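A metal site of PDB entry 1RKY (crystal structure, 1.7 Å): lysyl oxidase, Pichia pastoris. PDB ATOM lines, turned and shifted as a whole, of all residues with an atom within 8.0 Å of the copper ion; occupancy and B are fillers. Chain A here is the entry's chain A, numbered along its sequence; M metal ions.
The backbone NH of His 490 sits at hydrogen-bond distance from the backbone carbonyl oxygen of Leu 652, 2.9 Å away. NE2 of His 654 sits at hydrogen-bond distance from OD1 of Asp 660, at 2.9 Å. ND1 of His 488 is in hydrogen-bond range of O of Ser 486 (2.9 Å). O2 of TPQ 438 is in hydrogen-bond range of the side-chain amide nitrogen (ND2) of Asn 437 (2.8 Å).
Within 4 Å of the copper ion: TPQ 438, His 488, His 490 and His 654. The nearest printed residue that does not touch the copper ion is Leu 652 (4.9 Å).
The copper ion is bound by ND1 of His 654, NE2 of His 488, NE2 of His 490 and O4 of TPQ 438. The copper ion has four donor atoms within binding distance.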
ATOM      1  N   ALA A 342      -6.978  30.173  -2.079  1.00  0.00           N
ATOM      2  CA  ALA A 342      -8.079  30.107  -3.003  1.00  0.00           C
ATOM      3  C   ALA A 342      -9.228  30.862  -2.368  1.00  0.00           C
ATOM      4  O   ALA A 342      -9.807  30.427  -1.367  1.00  0.00           O
ATOM      5  CB  ALA A 342      -8.467  28.675  -3.303  1.00  0.00           C
ATOM      6  N   TYR A 344     -12.856  32.765  -2.946  1.00  0.00           N
ATOM      7  CA  TYR A 344     -14.018  32.716  -3.812  1.00  0.00           C
ATOM      8  C   TYR A 344     -14.913  33.925  -3.649  1.00  0.00           C
ATOM      9  O   TYR A 344     -15.003  34.509  -2.555  1.00  0.00           O
ATOM     10  CB  TYR A 344     -14.827  31.425  -3.511  1.00  0.00           C
ATOM     11  CG  TYR A 344     -14.136  30.149  -3.958  1.00  0.00           C
ATOM     12  CD1 TYR A 344     -13.014  29.689  -3.303  1.00  0.00           C
ATOM     13  CD2 TYR A 344     -14.609  29.396  -5.066  1.00  0.00           C
ATOM     14  CE1 TYR A 344     -12.359  28.518  -3.737  1.00  0.00           C
ATOM     15  CE2 TYR A 344     -13.954  28.284  -5.475  1.00  0.00           C
ATOM     16  CZ  TYR A 344     -12.819  27.846  -4.806  1.00  0.00           C
ATOM     17  OH  TYR A 344     -12.163  26.720  -5.241  1.00  0.00           O
ATOM     18  N   ASN A 437     -10.019  18.548  -3.631  1.00  0.00           N
ATOM     19  CA  ASN A 437     -10.452  18.648  -5.019  1.00  0.00           C
ATOM     20  C   ASN A 437      -9.364  19.096  -5.990  1.00  0.00           C
ATOM     21  O   ASN A 437      -9.483  18.858  -7.195  1.00  0.00           O
ATOM     22  CB  ASN A 437     -11.692  19.578  -5.156  1.00  0.00           C
ATOM     23  CG  ASN A 437     -11.495  20.947  -4.538  1.00  0.00           C
ATOM     24  OD1 ASN A 437     -11.227  21.055  -3.342  1.00  0.00           O
ATOM     25  ND2 ASN A 437     -11.682  22.015  -5.339  1.00  0.00           N
ATOM     26  N   TPQ A 438      -8.411  19.886  -5.453  1.00  0.00           N
ATOM     27  CA  TPQ A 438      -7.392  20.569  -6.325  1.00  0.00           C
ATOM     28  CB  TPQ A 438      -7.063  21.997  -5.833  1.00  0.00           C
ATOM     29  C   TPQ A 438      -6.177  19.686  -6.495  1.00  0.00           C
ATOM     30  O   TPQ A 438      -5.661  19.144  -5.524  1.00  0.00           O
ATOM     31  C1  TPQ A 438      -7.977  22.905  -6.662  1.00  0.00           C
ATOM     32  C2  TPQ A 438      -9.129  23.649  -6.075  1.00  0.00           C
ATOM     33  O2  TPQ A 438      -9.373  23.575  -4.855  1.00  0.00           O
ATOM     34  C3  TPQ A 438     -10.001  24.496  -6.947  1.00  0.00           C
ATOM     35  C4  TPQ A 438      -9.759  24.600  -8.328  1.00  0.00           C
ATOM     36  O4  TPQ A 438     -10.468  25.290  -9.083  1.00  0.00           O
ATOM     37  C5  TPQ A 438      -8.607  23.856  -8.915  1.00  0.00           C
ATOM     38  O5  TPQ A 438      -8.385  23.957 -10.144  1.00  0.00           O
ATOM     39  C6  TPQ A 438      -7.745  23.014  -8.035  1.00  0.00           C
ATOM     40  N   TYR A 440      -2.327  20.488  -7.563  1.00  0.00           N
ATOM     41  CA  TYR A 440      -1.272  21.453  -7.905  1.00  0.00           C
ATOM     42  C   TYR A 440       0.029  20.767  -8.380  1.00  0.00           C
ATOM     43  O   TYR A 440       0.568  19.867  -7.732  1.00  0.00           O
ATOM     44  CB  TYR A 440      -0.952  22.343  -6.698  1.00  0.00           C
ATOM     45  CG  TYR A 440      -2.125  23.173  -6.221  1.00  0.00           C
ATOM     46  CD1 TYR A 440      -2.469  24.346  -6.844  1.00  0.00           C
ATOM     47  CD2 TYR A 440      -2.874  22.756  -5.105  1.00  0.00           C
ATOM     48  CE1 TYR A 440      -3.560  25.105  -6.402  1.00  0.00           C
ATOM     49  CE2 TYR A 440      -3.956  23.506  -4.658  1.00  0.00           C
ATOM     50  CZ  TYR A 440      -4.298  24.665  -5.307  1.00  0.00           C
ATOM     51  OH  TYR A 440      -5.371  25.405  -4.854  1.00  0.00           O
ATOM     52  N   ALA A 458      -2.582  23.993 -12.372  1.00  0.00           N
ATOM     53  CA  ALA A 458      -3.651  23.486 -11.528  1.00  0.00           C
ATOM     54  C   ALA A 458      -4.612  22.659 -12.357  1.00  0.00           C
ATOM     55  O   ALA A 458      -4.841  22.903 -13.551  1.00  0.00           O
ATOM     56  CB  ALA A 458      -4.366  24.604 -10.886  1.00  0.00           C
ATOM     57  N   ALA A 459      -5.176  21.633 -11.719  1.00  0.00           N
ATOM     58  CA  ALA A 459      -6.156  20.769 -12.347  1.00  0.00           C
ATOM     59  C   ALA A 459      -7.059  20.240 -11.227  1.00  0.00           C
ATOM     60  O   ALA A 459      -6.982  20.736 -10.106  1.00  0.00           O
ATOM     61  CB  ALA A 459      -5.491  19.620 -13.113  1.00  0.00           C
ATOM     62  N   GLY A 460      -7.912  19.285 -11.535  1.00  0.00           N
ATOM     63  CA  GLY A 460      -8.814  18.734 -10.540  1.00  0.00           C
ATOM     64  C   GLY A 460     -10.240  19.222 -10.668  1.00  0.00           C
ATOM     65  O   GLY A 460     -10.641  19.705 -11.712  1.00  0.00           O
ATOM     66  N   TYR A 461     -11.025  18.987  -9.628  1.00  0.00           N
ATOM     67  CA  TYR A 461     -12.417  19.412  -9.594  1.00  0.00           C
ATOM     68  C   TYR A 461     -12.514  20.823  -9.044  1.00  0.00           C
ATOM     69  O   TYR A 461     -11.921  21.149  -8.019  1.00  0.00           O
ATOM     70  CB  TYR A 461     -13.238  18.503  -8.666  1.00  0.00           C
ATOM     71  CG  TYR A 461     -13.585  17.157  -9.247  1.00  0.00           C
ATOM     72  CD1 TYR A 461     -12.949  15.986  -8.817  1.00  0.00           C
ATOM     73  CD2 TYR A 461     -14.540  17.053 -10.242  1.00  0.00           C
ATOM     74  CE1 TYR A 461     -13.275  14.753  -9.378  1.00  0.00           C
ATOM     75  CE2 TYR A 461     -14.863  15.829 -10.792  1.00  0.00           C
ATOM     76  CZ  TYR A 461     -14.241  14.672 -10.352  1.00  0.00           C
ATOM     77  OH  TYR A 461     -14.570  13.470 -10.912  1.00  0.00           O
ATOM     78  N   ILE A 462     -13.322  21.650  -9.701  1.00  0.00           N
ATOM     79  CA  ILE A 462     -13.610  22.966  -9.182  1.00  0.00           C
ATOM     80  C   ILE A 462     -14.565  22.912  -7.981  1.00  0.00           C
ATOM     81  O   ILE A 462     -15.341  21.967  -7.872  1.00  0.00           O
ATOM     82  CB  ILE A 462     -14.220  23.857 -10.276  1.00  0.00           C
ATOM     83  CG1 ILE A 462     -15.552  23.294 -10.782  1.00  0.00           C
ATOM     84  CG2 ILE A 462     -13.256  24.024 -11.436  1.00  0.00           C
ATOM     85  CD1 ILE A 462     -16.334  24.261 -11.611  1.00  0.00           C
ATOM     86  N   GLN A 463     -14.503  23.918  -7.119  1.00  0.00           N
ATOM     87  CA  GLN A 463     -15.527  24.092  -6.094  1.00  0.00           C
ATOM     88  C   GLN A 463     -16.615  24.951  -6.718  1.00  0.00           C
ATOM     89  O   GLN A 463     -16.550  26.180  -6.723  1.00  0.00           O
ATOM     90  CB  GLN A 463     -14.988  24.768  -4.847  1.00  0.00           C
ATOM     91  CG  GLN A 463     -16.059  25.008  -3.763  1.00  0.00           C
ATOM     92  CD  GLN A 463     -15.457  25.513  -2.485  1.00  0.00           C
ATOM     93  OE1 GLN A 463     -14.479  24.947  -2.009  1.00  0.00           O
ATOM     94  NE2 GLN A 463     -16.062  26.554  -1.899  1.00  0.00           N
ATOM     95  N   SER A 486     -18.182  28.837  -9.840  1.00  0.00           N
ATOM     96  CA  SER A 486     -17.884  29.967  -8.957  1.00  0.00           C
ATOM     97  C   SER A 486     -16.498  30.609  -9.191  1.00  0.00           C
ATOM     98  O   SER A 486     -15.480  29.940  -9.318  1.00  0.00           O
ATOM     99  CB  SER A 486     -18.068  29.538  -7.502  1.00  0.00           C
ATOM    100  OG  SER A 486     -19.446  29.268  -7.255  1.00  0.00           O
ATOM    101  N   PHE A 487     -16.536  31.920  -9.234  1.00  0.00           N
ATOM    102  CA  PHE A 487     -15.387  32.735  -9.582  1.00  0.00           C
ATOM    103  C   PHE A 487     -14.409  32.777  -8.403  1.00  0.00           C
ATOM    104  O   PHE A 487     -14.840  32.965  -7.272  1.00  0.00           O
ATOM    105  CB  PHE A 487     -15.949  34.114  -9.869  1.00  0.00           C
ATOM    106  CG  PHE A 487     -14.963  35.152 -10.249  1.00  0.00           C
ATOM    107  CD1 PHE A 487     -15.220  36.481  -9.952  1.00  0.00           C
ATOM    108  CD2 PHE A 487     -13.825  34.842 -10.969  1.00  0.00           C
ATOM    109  CE1 PHE A 487     -14.339  37.468 -10.327  1.00  0.00           C
ATOM    110  CE2 PHE A 487     -12.928  35.842 -11.331  1.00  0.00           C
ATOM    111  CZ  PHE A 487     -13.177  37.142 -10.991  1.00  0.00           C
ATOM    112  N   HIS A 488     -13.120  32.527  -8.625  1.00  0.00           N
ATOM    113  CA  HIS A 488     -12.158  32.496  -7.521  1.00  0.00           C
ATOM    114  C   HIS A 488     -10.769  32.879  -7.979  1.00  0.00           C
ATOM    115  O   HIS A 488     -10.450  32.799  -9.177  1.00  0.00           O
ATOM    116  CB  HIS A 488     -12.119  31.150  -6.830  1.00  0.00           C
ATOM    117  CG  HIS A 488     -11.793  30.011  -7.730  1.00  0.00           C
ATOM    118  ND1 HIS A 488     -12.725  29.481  -8.610  1.00  0.00           N
ATOM    119  CD2 HIS A 488     -10.662  29.293  -7.890  1.00  0.00           C
ATOM    120  CE1 HIS A 488     -12.162  28.478  -9.278  1.00  0.00           C
ATOM    121  NE2 HIS A 488     -10.913  28.355  -8.861  1.00  0.00           N
ATOM    122  N   ASP A 489      -9.974  33.352  -7.032  1.00  0.00           N
ATOM    123  CA  ASP A 489      -8.576  33.630  -7.283  1.00  0.00           C
ATOM    124  C   ASP A 489      -7.731  32.560  -6.648  1.00  0.00           C
ATOM    125  O   ASP A 489      -7.976  32.179  -5.510  1.00  0.00           O
ATOM    126  CB  ASP A 489      -8.211  34.956  -6.639  1.00  0.00           C
ATOM    127  CG  ASP A 489      -8.503  36.136  -7.514  1.00  0.00           C
ATOM    128  OD1 ASP A 489      -8.757  35.990  -8.757  1.00  0.00           O
ATOM    129  OD2 ASP A 489      -8.476  37.273  -7.002  1.00  0.00           O
ATOM    130  N   HIS A 490      -6.722  32.084  -7.370  1.00  0.00           N
ATOM    131  CA  HIS A 490      -5.652  31.305  -6.785  1.00  0.00           C
ATOM    132  C   HIS A 490      -4.453  32.259  -6.709  1.00  0.00           C
ATOM    133  O   HIS A 490      -4.165  32.954  -7.685  1.00  0.00           O
ATOM    134  CB  HIS A 490      -5.219  30.180  -7.715  1.00  0.00           C
ATOM    135  CG  HIS A 490      -6.262  29.157  -7.980  1.00  0.00           C
ATOM    136  ND1 HIS A 490      -6.415  28.040  -7.174  1.00  0.00           N
ATOM    137  CD2 HIS A 490      -7.143  29.019  -8.993  1.00  0.00           C
ATOM    138  CE1 HIS A 490      -7.387  27.288  -7.672  1.00  0.00           C
ATOM    139  NE2 HIS A 490      -7.823  27.850  -8.777  1.00  0.00           N
ATOM    140  N   LEU A 652      -3.961  33.082 -10.623  1.00  0.00           N
ATOM    141  CA  LEU A 652      -4.929  32.833 -11.669  1.00  0.00           C
ATOM    142  C   LEU A 652      -6.275  33.344 -11.221  1.00  0.00           C
ATOM    143  O   LEU A 652      -6.683  32.998 -10.111  1.00  0.00           O
ATOM    144  CB  LEU A 652      -5.049  31.328 -11.905  1.00  0.00           C
ATOM    145  CG  LEU A 652      -6.183  30.869 -12.836  1.00  0.00           C
ATOM    146  CD1 LEU A 652      -6.001  31.476 -14.217  1.00  0.00           C
ATOM    147  CD2 LEU A 652      -6.298  29.325 -12.913  1.00  0.00           C
ATOM    148  N   HIS A 653      -6.938  34.166 -12.036  1.00  0.00           N
ATOM    149  CA  HIS A 653      -8.330  34.494 -11.837  1.00  0.00           C
ATOM    150  C   HIS A 653      -9.130  33.423 -12.596  1.00  0.00           C
ATOM    151  O   HIS A 653      -9.156  33.437 -13.838  1.00  0.00           O
ATOM    152  CB  HIS A 653      -8.664  35.842 -12.445  1.00  0.00           C
ATOM    153  CG  HIS A 653      -7.771  36.958 -11.982  1.00  0.00           C
ATOM    154  ND1 HIS A 653      -7.543  37.238 -10.658  1.00  0.00           N
ATOM    155  CD2 HIS A 653      -7.046  37.874 -12.688  1.00  0.00           C
ATOM    156  CE1 HIS A 653      -6.759  38.298 -10.562  1.00  0.00           C
ATOM    157  NE2 HIS A 653      -6.436  38.696 -11.784  1.00  0.00           N
ATOM    158  N   HIS A 654      -9.768  32.514 -11.880  1.00  0.00           N
ATOM    159  CA  HIS A 654     -10.358  31.361 -12.532  1.00  0.00           C
ATOM    160  C   HIS A 654     -11.872  31.535 -12.589  1.00  0.00           C
ATOM    161  O   HIS A 654     -12.500  31.622 -11.559  1.00  0.00           O
ATOM    162  CB  HIS A 654      -9.986  30.149 -11.718  1.00  0.00           C
ATOM    163  CG  HIS A 654     -10.182  28.840 -12.399  1.00  0.00           C
ATOM    164  ND1 HIS A 654      -9.979  27.641 -11.746  1.00  0.00           N
ATOM    165  CD2 HIS A 654     -10.600  28.528 -13.655  1.00  0.00           C
ATOM    166  CE1 HIS A 654     -10.268  26.642 -12.575  1.00  0.00           C
ATOM    167  NE2 HIS A 654     -10.616  27.155 -13.746  1.00  0.00           N
ATOM    168  N   LEU A 655     -12.422  31.591 -13.802  1.00  0.00           N
ATOM    169  CA  LEU A 655     -13.856  31.664 -14.030  1.00  0.00           C
ATOM    170  C   LEU A 655     -14.197  30.373 -14.816  1.00  0.00           C
ATOM    171  O   LEU A 655     -14.065  30.373 -16.038  1.00  0.00           O
ATOM    172  CB  LEU A 655     -14.201  32.911 -14.816  1.00  0.00           C
ATOM    173  CG  LEU A 655     -15.702  33.123 -15.083  1.00  0.00           C
ATOM    174  CD1 LEU A 655     -16.467  33.424 -13.804  1.00  0.00           C
ATOM    175  CD2 LEU A 655     -15.931  34.183 -16.127  1.00  0.00           C
ATOM    176  N   PRO A 656     -14.500  29.274 -14.123  1.00  0.00           N
ATOM    177  CA  PRO A 656     -14.699  27.997 -14.803  1.00  0.00           C
ATOM    178  C   PRO A 656     -15.799  28.035 -15.829  1.00  0.00           C
ATOM    179  O   PRO A 656     -16.809  28.715 -15.647  1.00  0.00           O
ATOM    180  CB  PRO A 656     -15.022  27.027 -13.659  1.00  0.00           C
ATOM    181  CG  PRO A 656     -14.330  27.652 -12.464  1.00  0.00           C
ATOM    182  CD  PRO A 656     -14.567  29.074 -12.671  1.00  0.00           C
ATOM    183  N   ASP A 660     -13.786  23.254 -17.933  1.00  0.00           N
ATOM    184  CA  ASP A 660     -13.417  22.795 -16.603  1.00  0.00           C
ATOM    185  C   ASP A 660     -14.297  21.634 -16.102  1.00  0.00           C
ATOM    186  O   ASP A 660     -14.223  21.272 -14.928  1.00  0.00           O
ATOM    187  CB  ASP A 660     -13.507  23.940 -15.605  1.00  0.00           C
ATOM    188  CG  ASP A 660     -12.550  25.083 -15.926  1.00  0.00           C
ATOM    189  OD1 ASP A 660     -11.366  24.984 -15.524  1.00  0.00           O
ATOM    190  OD2 ASP A 660     -12.890  26.086 -16.562  1.00  0.00           O
ATOM    191  N   THR A 664     -10.741  20.740 -14.438  1.00  0.00           N
ATOM    192  CA  THR A 664      -9.834  21.730 -14.957  1.00  0.00           C
ATOM    193  C   THR A 664      -8.577  21.094 -15.561  1.00  0.00           C
ATOM    194  O   THR A 664      -8.086  20.088 -15.038  1.00  0.00           O
ATOM    195  CB  THR A 664      -9.447  22.640 -13.774  1.00  0.00           C
ATOM    196  OG1 THR A 664     -10.605  23.378 -13.345  1.00  0.00           O
ATOM    197  CG2 THR A 664      -8.428  23.683 -14.215  1.00  0.00           C
ATOM    198  N   ALA A 669      -4.207  26.484 -17.091  1.00  0.00           N
ATOM    199  CA  ALA A 669      -4.230  26.956 -15.720  1.00  0.00           C
ATOM    200  C   ALA A 669      -2.773  26.969 -15.236  1.00  0.00           C
ATOM    201  O   ALA A 669      -2.363  26.061 -14.529  1.00  0.00           O
ATOM    202  CB  ALA A 669      -5.058  26.040 -14.861  1.00  0.00           C
HETATM  203 CU    CU M   1      -9.502  27.317  -9.849  1.00  0.00          CU
